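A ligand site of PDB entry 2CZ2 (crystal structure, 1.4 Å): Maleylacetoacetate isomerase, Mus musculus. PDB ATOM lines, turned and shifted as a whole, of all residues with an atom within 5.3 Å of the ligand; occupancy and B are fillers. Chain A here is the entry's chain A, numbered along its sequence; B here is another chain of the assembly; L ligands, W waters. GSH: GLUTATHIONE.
NH1 of Arg 26 is in hydrogen-bond range of OG of Ser 79, 2.9 Å away. The backbone carbonyl oxygen of Leu 45 is in hydrogen-bond range of the side-chain amide nitrogen of Gln 52. OG of Ser 124 lies within hydrogen-bond range of ND2 of Asn 122 (3.3 Å). The side-chain sulfur of Cys 23 sits at hydrogen-bond distance from the guanidinium group of Arg 26. N of Cys 23 sits close to OG of Ser 21 (3.5 Å). The side-chain hydroxyl (OG) of Ser 21 is in hydrogen-bond range of the side-chain hydroxyl (OG) of Ser 24, at 2.9 Å. NE2 of Gln 118 sits close to SG of Cys 23 (3.7 Å).
Merely in contact with the ligand: Gln 65 (3.1 Å), Leu 123 (3.4 Å), Pro 67 (3.6 Å), Ser 115 of chain B (3.7 Å), Leu 45 (3.7 Å), Lys 64 (3.8 Å) and Phe 53 (3.8 Å). Hydrophobic or aromatic side chains within 4 Å of the ligand: Leu 45, Phe 53, Val 66, Pro 67 and Leu 123. Of the 24 residues printed, 18 come within 4 Å of the ligand. Along chain A the residues within 4 Å of the ligand span positions 21 to 124.
Water W4 bridges OE1 of the ligand (2.6 Å) and OE1 of Gln 118 (2.8 Å). Water W7 lies within hydrogen-bond range of O11 of the ligand, O of Pro 67 and N of Gln 78. Water W3 lies within hydrogen-bond range of the side-chain amide oxygen of Gln 78 (2.8 Å), the backbone NH of Leu 80 (3.0 Å), the side-chain carboxylate of Asp 111 of chain B (3.1 Å), an oxygen (O12) of the ligand (3.2 Å) and the backbone NH of Ser 79 (3.5 Å). Water W1 lies within hydrogen-bond range of NE2 of Gln 65 (2.8 Å), OG of Ser 124 (2.9 Å), ND2 of Asn 122 (3.1 Å) and O32 of the ligand (3.3 Å). Water W6 lies within hydrogen-bond range of the side-chain hydroxyl of Ser 115 of chain B (2.6 Å) and a nitrogen (N1) of the ligand (3.3 Å). Water W5 lies within hydrogen-bond range of the backbone carbonyl oxygen of Ala 114 (2.7 Å), the side-chain amide oxygen of Gln 118 (2.9 Å), the guanidinium group of Arg 26 (3.0 Å), a nitrogen (N1) of the ligand (3.4 Å) and the side-chain sulfur of Cys 23 (3.7 Å).
N of Ser 79 sits at hydrogen-bond distance from O11 of the ligand. An oxygen (O12) of the ligand is in hydrogen-bond range of the side-chain hydroxyl (OG) of Ser 79, 2.5 Å away. The backbone NH (N) of Val 66 sits at hydrogen-bond distance from an oxygen (O2) of the ligand. O of Val 66 sits at hydrogen-bond distance from N2 of the ligand (2.8 Å). An oxygen (O31) of the ligand sits at hydrogen-bond distance from the side-chain amide nitrogen (NE2) of Gln 52, 2.8 Å away. O32 of the ligand is in hydrogen-bond range of N of Ser 124, 2.9 Å away. An oxygen (O32) of the ligand lies close to the side-chain hydroxyl (OG) of Ser 124 (3.4 Å). N1 of the ligand sits at hydrogen-bond distance from OE1 of Gln 78 (2.9 Å). The side-chain amide oxygen of Asn 122 is in hydrogen-bond range of a nitrogen (N3) of the ligand (3.0 Å). An oxygen (O12) of the ligand lies within salt-bridge range of the guanidinium group (NH1) of Arg 26 (3.0 Å). The side-chain hydroxyl (OG) of Ser 21 lies close to a sulfur (SG2) of the ligand (3.1 Å). The side-chain amide nitrogen of Gln 118 is in hydrogen-bond range of an oxygen (OE1) of the ligand (3.3 Å). The backbone NH (N) of Cys 23 sits close to a sulfur (SG2) of the ligand (3.6 Å). SG of Cys 23 lies close to SG2 of the ligand, at 3.5 Å. A sulfur (SG2) of the ligand sits close to the backbone NH (N) of Ser 22 (3.8 Å).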
ATOM      1  N   SER A  21      22.771   1.857 -10.522  1.00  0.00           N
ATOM      2  CA  SER A  21      22.678   3.252 -10.982  1.00  0.00           C
ATOM      3  C   SER A  21      21.297   3.815 -10.718  1.00  0.00           C
ATOM      4  O   SER A  21      20.315   3.290 -11.253  1.00  0.00           O
ATOM      5  CB  SER A  21      22.977   3.295 -12.488  1.00  0.00           C
ATOM      6  OG  SER A  21      22.468   4.484 -13.111  1.00  0.00           O
ATOM      7  N   SER A  22      21.213   4.894  -9.935  1.00  0.00           N
ATOM      8  CA  SER A  22      19.932   5.568  -9.706  1.00  0.00           C
ATOM      9  C   SER A  22      19.300   6.078 -11.006  1.00  0.00           C
ATOM     10  O   SER A  22      18.107   5.925 -11.221  1.00  0.00           O
ATOM     11  CB  SER A  22      20.043   6.686  -8.658  1.00  0.00           C
ATOM     12  OG  SER A  22      20.815   7.779  -9.134  1.00  0.00           O
ATOM     13  N   CYS A  23      20.099   6.677 -11.876  1.00  0.00           N
ATOM     14  CA  CYS A  23      19.574   7.256 -13.116  1.00  0.00           C
ATOM     15  C   CYS A  23      19.054   6.191 -14.046  1.00  0.00           C
ATOM     16  O   CYS A  23      18.104   6.416 -14.755  1.00  0.00           O
ATOM     17  CB  CYS A  23      20.670   8.051 -13.809  1.00  0.00           C
ATOM     18  SG  CYS A  23      21.340   9.363 -12.771  1.00  0.00           S
ATOM     19  N   SER A  24      19.713   5.040 -14.061  1.00  0.00           N
ATOM     20  CA  SER A  24      19.219   3.907 -14.836  1.00  0.00           C
ATOM     21  C   SER A  24      17.903   3.379 -14.289  1.00  0.00           C
ATOM     22  O   SER A  24      16.986   3.058 -15.052  1.00  0.00           O
ATOM     23  CB  SER A  24      20.248   2.764 -14.826  1.00  0.00           C
ATOM     24  OG  SER A  24      21.477   3.144 -15.446  1.00  0.00           O
ATOM     25  N   ARG A  26      15.603   4.994 -12.843  1.00  0.00           N
ATOM     26  CA  ARG A  26      14.548   5.909 -13.302  1.00  0.00           C
ATOM     27  C   ARG A  26      13.950   5.451 -14.603  1.00  0.00           C
ATOM     28  O   ARG A  26      12.745   5.416 -14.795  1.00  0.00           O
ATOM     29  CB  ARG A  26      15.068   7.347 -13.503  1.00  0.00           C
ATOM     30  CG  ARG A  26      15.591   8.074 -12.294  1.00  0.00           C
ATOM     31  CD  ARG A  26      16.314   9.350 -12.725  1.00  0.00           C
ATOM     32  NE  ARG A  26      17.075   9.957 -11.654  1.00  0.00           N
ATOM     33  CZ  ARG A  26      18.018  10.888 -11.803  1.00  0.00           C
ATOM     34  NH1 ARG A  26      18.327  11.351 -13.024  1.00  0.00           N
ATOM     35  NH2 ARG A  26      18.697  11.330 -10.743  1.00  0.00           N
ATOM     36  N   LEU A  45      29.931  -0.040 -13.935  1.00  0.00           N
ATOM     37  CA  LEU A  45      30.517   1.276 -13.691  1.00  0.00           C
ATOM     38  C   LEU A  45      31.729   1.274 -12.789  1.00  0.00           C
ATOM     39  O   LEU A  45      32.368   2.295 -12.668  1.00  0.00           O
ATOM     40  CB  LEU A  45      29.447   2.224 -13.123  1.00  0.00           C
ATOM     41  CG  LEU A  45      28.219   2.503 -13.991  1.00  0.00           C
ATOM     42  CD1 LEU A  45      27.327   3.501 -13.255  1.00  0.00           C
ATOM     43  CD2 LEU A  45      28.582   3.053 -15.393  1.00  0.00           C
ATOM     44  N   GLN A  52      32.146   2.342 -18.724  1.00  0.00           N
ATOM     45  CA  GLN A  52      31.686   3.597 -19.291  1.00  0.00           C
ATOM     46  C   GLN A  52      32.850   4.390 -19.924  1.00  0.00           C
ATOM     47  O   GLN A  52      32.615   5.307 -20.673  1.00  0.00           O
ATOM     48  CB  GLN A  52      30.942   4.442 -18.230  1.00  0.00           C
ATOM     49  CG  GLN A  52      31.804   5.026 -17.094  1.00  0.00           C
ATOM     50  CD  GLN A  52      31.962   4.106 -15.882  1.00  0.00           C
ATOM     51  OE1 GLN A  52      32.003   2.877 -16.044  1.00  0.00           O
ATOM     52  NE2 GLN A  52      32.113   4.702 -14.684  1.00  0.00           N
ATOM     53  N   PHE A  53      34.079   4.019 -19.624  1.00  0.00           N
ATOM     54  CA  PHE A  53      35.238   4.675 -20.221  1.00  0.00           C
ATOM     55  C   PHE A  53      35.755   3.984 -21.475  1.00  0.00           C
ATOM     56  O   PHE A  53      36.690   4.510 -22.104  1.00  0.00           O
ATOM     57  CB  PHE A  53      36.329   4.809 -19.172  1.00  0.00           C
ATOM     58  CG  PHE A  53      35.924   5.682 -18.020  1.00  0.00           C
ATOM     59  CD1 PHE A  53      35.615   5.118 -16.803  1.00  0.00           C
ATOM     60  CD2 PHE A  53      35.814   7.067 -18.174  1.00  0.00           C
ATOM     61  CE1 PHE A  53      35.224   5.910 -15.728  1.00  0.00           C
ATOM     62  CE2 PHE A  53      35.414   7.879 -17.102  1.00  0.00           C
ATOM     63  CZ  PHE A  53      35.109   7.295 -15.874  1.00  0.00           C
ATOM     64  N   LYS A  64      30.052   9.568 -20.816  1.00  0.00           N
ATOM     65  CA  LYS A  64      30.569   8.398 -20.098  1.00  0.00           C
ATOM     66  C   LYS A  64      29.671   8.103 -18.878  1.00  0.00           C
ATOM     67  O   LYS A  64      30.139   7.813 -17.790  1.00  0.00           O
ATOM     68  CB  LYS A  64      32.014   8.631 -19.682  1.00  0.00           C
ATOM     69  CG  LYS A  64      32.943   8.865 -20.878  1.00  0.00           C
ATOM     70  CD  LYS A  64      34.260   9.463 -20.455  1.00  0.00           C
ATOM     71  CE  LYS A  64      34.602  10.679 -21.307  1.00  0.00           C
ATOM     72  NZ  LYS A  64      35.603  11.580 -20.623  1.00  0.00           N
ATOM     73  N   GLN A  65      28.366   8.128 -19.117  1.00  0.00           N
ATOM     74  CA  GLN A  65      27.385   7.841 -18.076  1.00  0.00           C
ATOM     75  C   GLN A  65      26.287   6.937 -18.618  1.00  0.00           C
ATOM     76  O   GLN A  65      26.001   6.940 -19.824  1.00  0.00           O
ATOM     77  CB  GLN A  65      26.758   9.145 -17.571  1.00  0.00           C
ATOM     78  CG  GLN A  65      27.755  10.053 -16.865  1.00  0.00           C
ATOM     79  CD  GLN A  65      27.254  11.438 -16.628  1.00  0.00           C
ATOM     80  OE1 GLN A  65      26.256  11.869 -17.225  1.00  0.00           O
ATOM     81  NE2 GLN A  65      27.953  12.187 -15.761  1.00  0.00           N
ATOM     82  N   VAL A  66      25.627   6.220 -17.708  1.00  0.00           N
ATOM     83  CA  VAL A  66      24.353   5.557 -18.002  1.00  0.00           C
ATOM     84  C   VAL A  66      23.243   6.328 -17.331  1.00  0.00           C
ATOM     85  O   VAL A  66      23.467   6.994 -16.341  1.00  0.00           O
ATOM     86  CB  VAL A  66      24.308   4.084 -17.539  1.00  0.00           C
ATOM     87  CG1 VAL A  66      25.267   3.223 -18.367  1.00  0.00           C
ATOM     88  CG2 VAL A  66      24.611   3.980 -16.081  1.00  0.00           C
ATOM     89  N   PRO A  67      22.013   6.260 -17.840  1.00  0.00           N
ATOM     90  CA  PRO A  67      21.591   5.428 -18.971  1.00  0.00           C
ATOM     91  C   PRO A  67      21.768   6.042 -20.331  1.00  0.00           C
ATOM     92  O   PRO A  67      21.923   7.244 -20.505  1.00  0.00           O
ATOM     93  CB  PRO A  67      20.089   5.257 -18.703  1.00  0.00           C
ATOM     94  CG  PRO A  67      19.705   6.538 -18.058  1.00  0.00           C
ATOM     95  CD  PRO A  67      20.859   6.900 -17.197  1.00  0.00           C
ATOM     96  N   GLN A  78      20.722  11.043 -21.092  1.00  0.00           N
ATOM     97  CA  GLN A  78      20.127  11.879 -20.053  1.00  0.00           C
ATOM     98  C   GLN A  78      18.752  11.325 -19.650  1.00  0.00           C
ATOM     99  O   GLN A  78      17.790  11.366 -20.421  1.00  0.00           O
ATOM    100  CB  GLN A  78      20.054  13.347 -20.451  1.00  0.00           C
ATOM    101  CG  GLN A  78      21.414  14.011 -20.528  1.00  0.00           C
ATOM    102  CD  GLN A  78      22.002  14.278 -19.167  1.00  0.00           C
ATOM    103  OE1 GLN A  78      21.272  14.330 -18.142  1.00  0.00           O
ATOM    104  NE2 GLN A  78      23.313  14.469 -19.122  1.00  0.00           N
ATOM    105  N   SER A  79      18.670  10.786 -18.444  1.00  0.00           N
ATOM    106  CA  SER A  79      17.483  10.079 -18.021  1.00  0.00           C
ATOM    107  C   SER A  79      16.192  10.928 -18.139  1.00  0.00           C
ATOM    108  O   SER A  79      15.156  10.402 -18.527  1.00  0.00           O
ATOM    109  CB  SER A  79      17.634   9.538 -16.605  1.00  0.00           C
ATOM    110  OG  SER A  79      17.803  10.567 -15.716  1.00  0.00           O
ATOM    111  N   LEU A  80      16.247  12.223 -17.813  1.00  0.00           N
ATOM    112  CA  LEU A  80      15.047  13.026 -17.925  1.00  0.00           C
ATOM    113  C   LEU A  80      14.682  13.315 -19.358  1.00  0.00           C
ATOM    114  O   LEU A  80      13.519  13.330 -19.697  1.00  0.00           O
ATOM    115  CB  LEU A  80      15.149  14.292 -17.104  1.00  0.00           C
ATOM    116  CG  LEU A  80      14.844  14.118 -15.612  1.00  0.00           C
ATOM    117  CD1 LEU A  80      15.674  13.072 -14.938  1.00  0.00           C
ATOM    118  CD2 LEU A  80      15.012  15.454 -14.919  1.00  0.00           C
ATOM    119  N   ALA A 114      17.434  15.387  -9.784  1.00  0.00           N
ATOM    120  CA  ALA A 114      18.287  14.987 -10.879  1.00  0.00           C
ATOM    121  C   ALA A 114      19.413  15.961 -11.203  1.00  0.00           C
ATOM    122  O   ALA A 114      20.433  15.550 -11.729  1.00  0.00           O
ATOM    123  CB  ALA A 114      17.477  14.669 -12.096  1.00  0.00           C
ATOM    124  N   GLN A 118      21.627  14.257  -7.207  1.00  0.00           N
ATOM    125  CA  GLN A 118      22.338  13.122  -7.809  1.00  0.00           C
ATOM    126  C   GLN A 118      23.718  13.501  -8.349  1.00  0.00           C
ATOM    127  O   GLN A 118      24.672  12.776  -8.089  1.00  0.00           O
ATOM    128  CB  GLN A 118      21.513  12.420  -8.879  1.00  0.00           C
ATOM    129  CG  GLN A 118      22.073  11.071  -9.376  1.00  0.00           C
ATOM    130  CD  GLN A 118      23.199  11.232 -10.386  1.00  0.00           C
ATOM    131  OE1 GLN A 118      23.247  12.240 -11.083  1.00  0.00           O
ATOM    132  NE2 GLN A 118      24.113  10.255 -10.465  1.00  0.00           N
ATOM    133  N   ASN A 122      27.425  11.459  -7.501  1.00  0.00           N
ATOM    134  CA  ASN A 122      27.769  10.542  -8.567  1.00  0.00           C
ATOM    135  C   ASN A 122      29.185   9.981  -8.353  1.00  0.00           C
ATOM    136  O   ASN A 122      30.042  10.630  -7.736  1.00  0.00           O
ATOM    137  CB  ASN A 122      27.668  11.268  -9.906  1.00  0.00           C
ATOM    138  CG  ASN A 122      27.922  10.383 -11.104  1.00  0.00           C
ATOM    139  OD1 ASN A 122      27.513   9.203 -11.140  1.00  0.00           O
ATOM    140  ND2 ASN A 122      28.546  10.950 -12.125  1.00  0.00           N
ATOM    141  N   LEU A 123      29.418   8.778  -8.881  1.00  0.00           N
ATOM    142  CA  LEU A 123      30.664   8.033  -8.728  1.00  0.00           C
ATOM    143  C   LEU A 123      31.873   8.875  -9.089  1.00  0.00           C
ATOM    144  O   LEU A 123      32.798   8.981  -8.294  1.00  0.00           O
ATOM    145  CB  LEU A 123      30.593   6.777  -9.611  1.00  0.00           C
ATOM    146  CG  LEU A 123      31.845   5.905  -9.647  1.00  0.00           C
ATOM    147  CD1 LEU A 123      32.159   5.384  -8.238  1.00  0.00           C
ATOM    148  CD2 LEU A 123      31.626   4.763 -10.627  1.00  0.00           C
ATOM    149  N   SER A 124      31.875   9.486 -10.265  1.00  0.00           N
ATOM    150  CA  SER A 124      33.016  10.264 -10.707  1.00  0.00           C
ATOM    151  C   SER A 124      33.307  11.458  -9.793  1.00  0.00           C
ATOM    152  O   SER A 124      34.460  11.836  -9.618  1.00  0.00           O
ATOM    153  CB  SER A 124      32.860  10.766 -12.134  1.00  0.00           C
ATOM    154  OG  SER A 124      31.746  11.616 -12.263  1.00  0.00           O
ATOM    155  N   VAL A 125      32.278  12.065  -9.228  1.00  0.00           N
ATOM    156  CA  VAL A 125      32.454  13.148  -8.276  1.00  0.00           C
ATOM    157  C   VAL A 125      33.019  12.631  -6.949  1.00  0.00           C
ATOM    158  O   VAL A 125      33.942  13.221  -6.395  1.00  0.00           O
ATOM    159  CB  VAL A 125      31.121  13.911  -8.056  1.00  0.00           C
ATOM    160  CG1 VAL A 125      31.245  14.930  -6.942  1.00  0.00           C
ATOM    161  CG2 VAL A 125      30.702  14.583  -9.341  1.00  0.00           C
ATOM    162  N   ASP B 111      20.288  19.180 -20.408  1.00  0.00           N
ATOM    163  CA  ASP B 111      20.543  18.426 -19.188  1.00  0.00           C
ATOM    164  C   ASP B 111      22.030  18.133 -18.978  1.00  0.00           C
ATOM    165  O   ASP B 111      22.500  18.161 -17.861  1.00  0.00           O
ATOM    166  CB  ASP B 111      19.769  17.101 -19.195  1.00  0.00           C
ATOM    167  CG  ASP B 111      18.284  17.231 -19.062  1.00  0.00           C
ATOM    168  OD1 ASP B 111      17.744  18.343 -18.762  1.00  0.00           O
ATOM    169  OD2 ASP B 111      17.575  16.190 -19.222  1.00  0.00           O
ATOM    170  N   SER B 115      22.485  19.575 -15.526  1.00  0.00           N
ATOM    171  CA  SER B 115      22.665  18.504 -14.545  1.00  0.00           C
ATOM    172  C   SER B 115      24.081  18.005 -14.504  1.00  0.00           C
ATOM    173  O   SER B 115      24.558  17.618 -13.450  1.00  0.00           O
ATOM    174  CB  SER B 115      21.765  17.312 -14.875  1.00  0.00           C
ATOM    175  OG  SER B 115      20.400  17.656 -14.783  1.00  0.00           O
ATOM    176  N   GLY B 116      24.779  18.015 -15.639  1.00  0.00           N
ATOM    177  CA  GLY B 116      26.107  17.384 -15.706  1.00  0.00           C
ATOM    178  C   GLY B 116      27.305  18.303 -15.485  1.00  0.00           C
ATOM    179  O   GLY B 116      28.394  17.821 -15.164  1.00  0.00           O
HETATM  180  N1  GSH L   1      22.007  13.676 -15.393  1.00  0.00           N
HETATM  181  CA1 GSH L   1      22.231  12.297 -15.722  1.00  0.00           C
HETATM  182  C1  GSH L   1      21.100  11.523 -16.193  1.00  0.00           C
HETATM  183  O11 GSH L   1      21.130  10.521 -17.124  1.00  0.00           O
HETATM  184  O12 GSH L   1      20.028  11.770 -15.509  1.00  0.00           O
HETATM  185  CB1 GSH L   1      23.399  11.681 -14.939  1.00  0.00           C
HETATM  186  CG1 GSH L   1      23.843  10.302 -15.411  1.00  0.00           C
HETATM  187  CD1 GSH L   1      24.775   9.705 -14.408  1.00  0.00           C
HETATM  188  OE1 GSH L   1      25.430  10.487 -13.493  1.00  0.00           O
HETATM  189  N2  GSH L   1      24.924   8.396 -14.361  1.00  0.00           N
HETATM  190  CA2 GSH L   1      25.803   7.726 -13.444  1.00  0.00           C
HETATM  191  C2  GSH L   1      27.052   7.244 -14.094  1.00  0.00           C
HETATM  192  O2  GSH L   1      26.958   6.570 -15.289  1.00  0.00           O
HETATM  193  CB2 GSH L   1      25.050   6.516 -12.913  1.00  0.00           C
HETATM  194  SG2 GSH L   1      23.704   6.987 -11.804  1.00  0.00           S
HETATM  195  N3  GSH L   1      28.210   7.532 -13.524  1.00  0.00           N
HETATM  196  CA3 GSH L   1      29.384   7.057 -14.188  1.00  0.00           C
HETATM  197  C3  GSH L   1      30.549   7.685 -13.509  1.00  0.00           C
HETATM  198  O31 GSH L   1      31.833   7.391 -13.956  1.00  0.00           O
HETATM  199  O32 GSH L   1      30.358   8.523 -12.545  1.00  0.00           O
HETATM  200  O   HOH W   1      30.296  11.019 -14.695  1.00  0.00           O
HETATM  201  O   HOH W   2      34.039   7.328 -12.189  1.00  0.00           O
HETATM  202  O   HOH W   3      18.594  14.048 -17.283  1.00  0.00           O
HETATM  203  O   HOH W   4      25.533  12.899 -12.557  1.00  0.00           O
HETATM  204  O   HOH W   5      20.743  12.972 -12.357  1.00  0.00           O
HETATM  205  O   HOH W   6      19.185  15.361 -15.072  1.00  0.00           O
HETATM  206  O   HOH W   7      22.617   9.698 -19.225  1.00  0.00           O
HETATM  207  O   HOH W   8      24.396  14.802 -14.248  1.00  0.00           O
HETATM  208  O   HOH W   9      31.864   9.175 -16.024  1.00  0.00           O
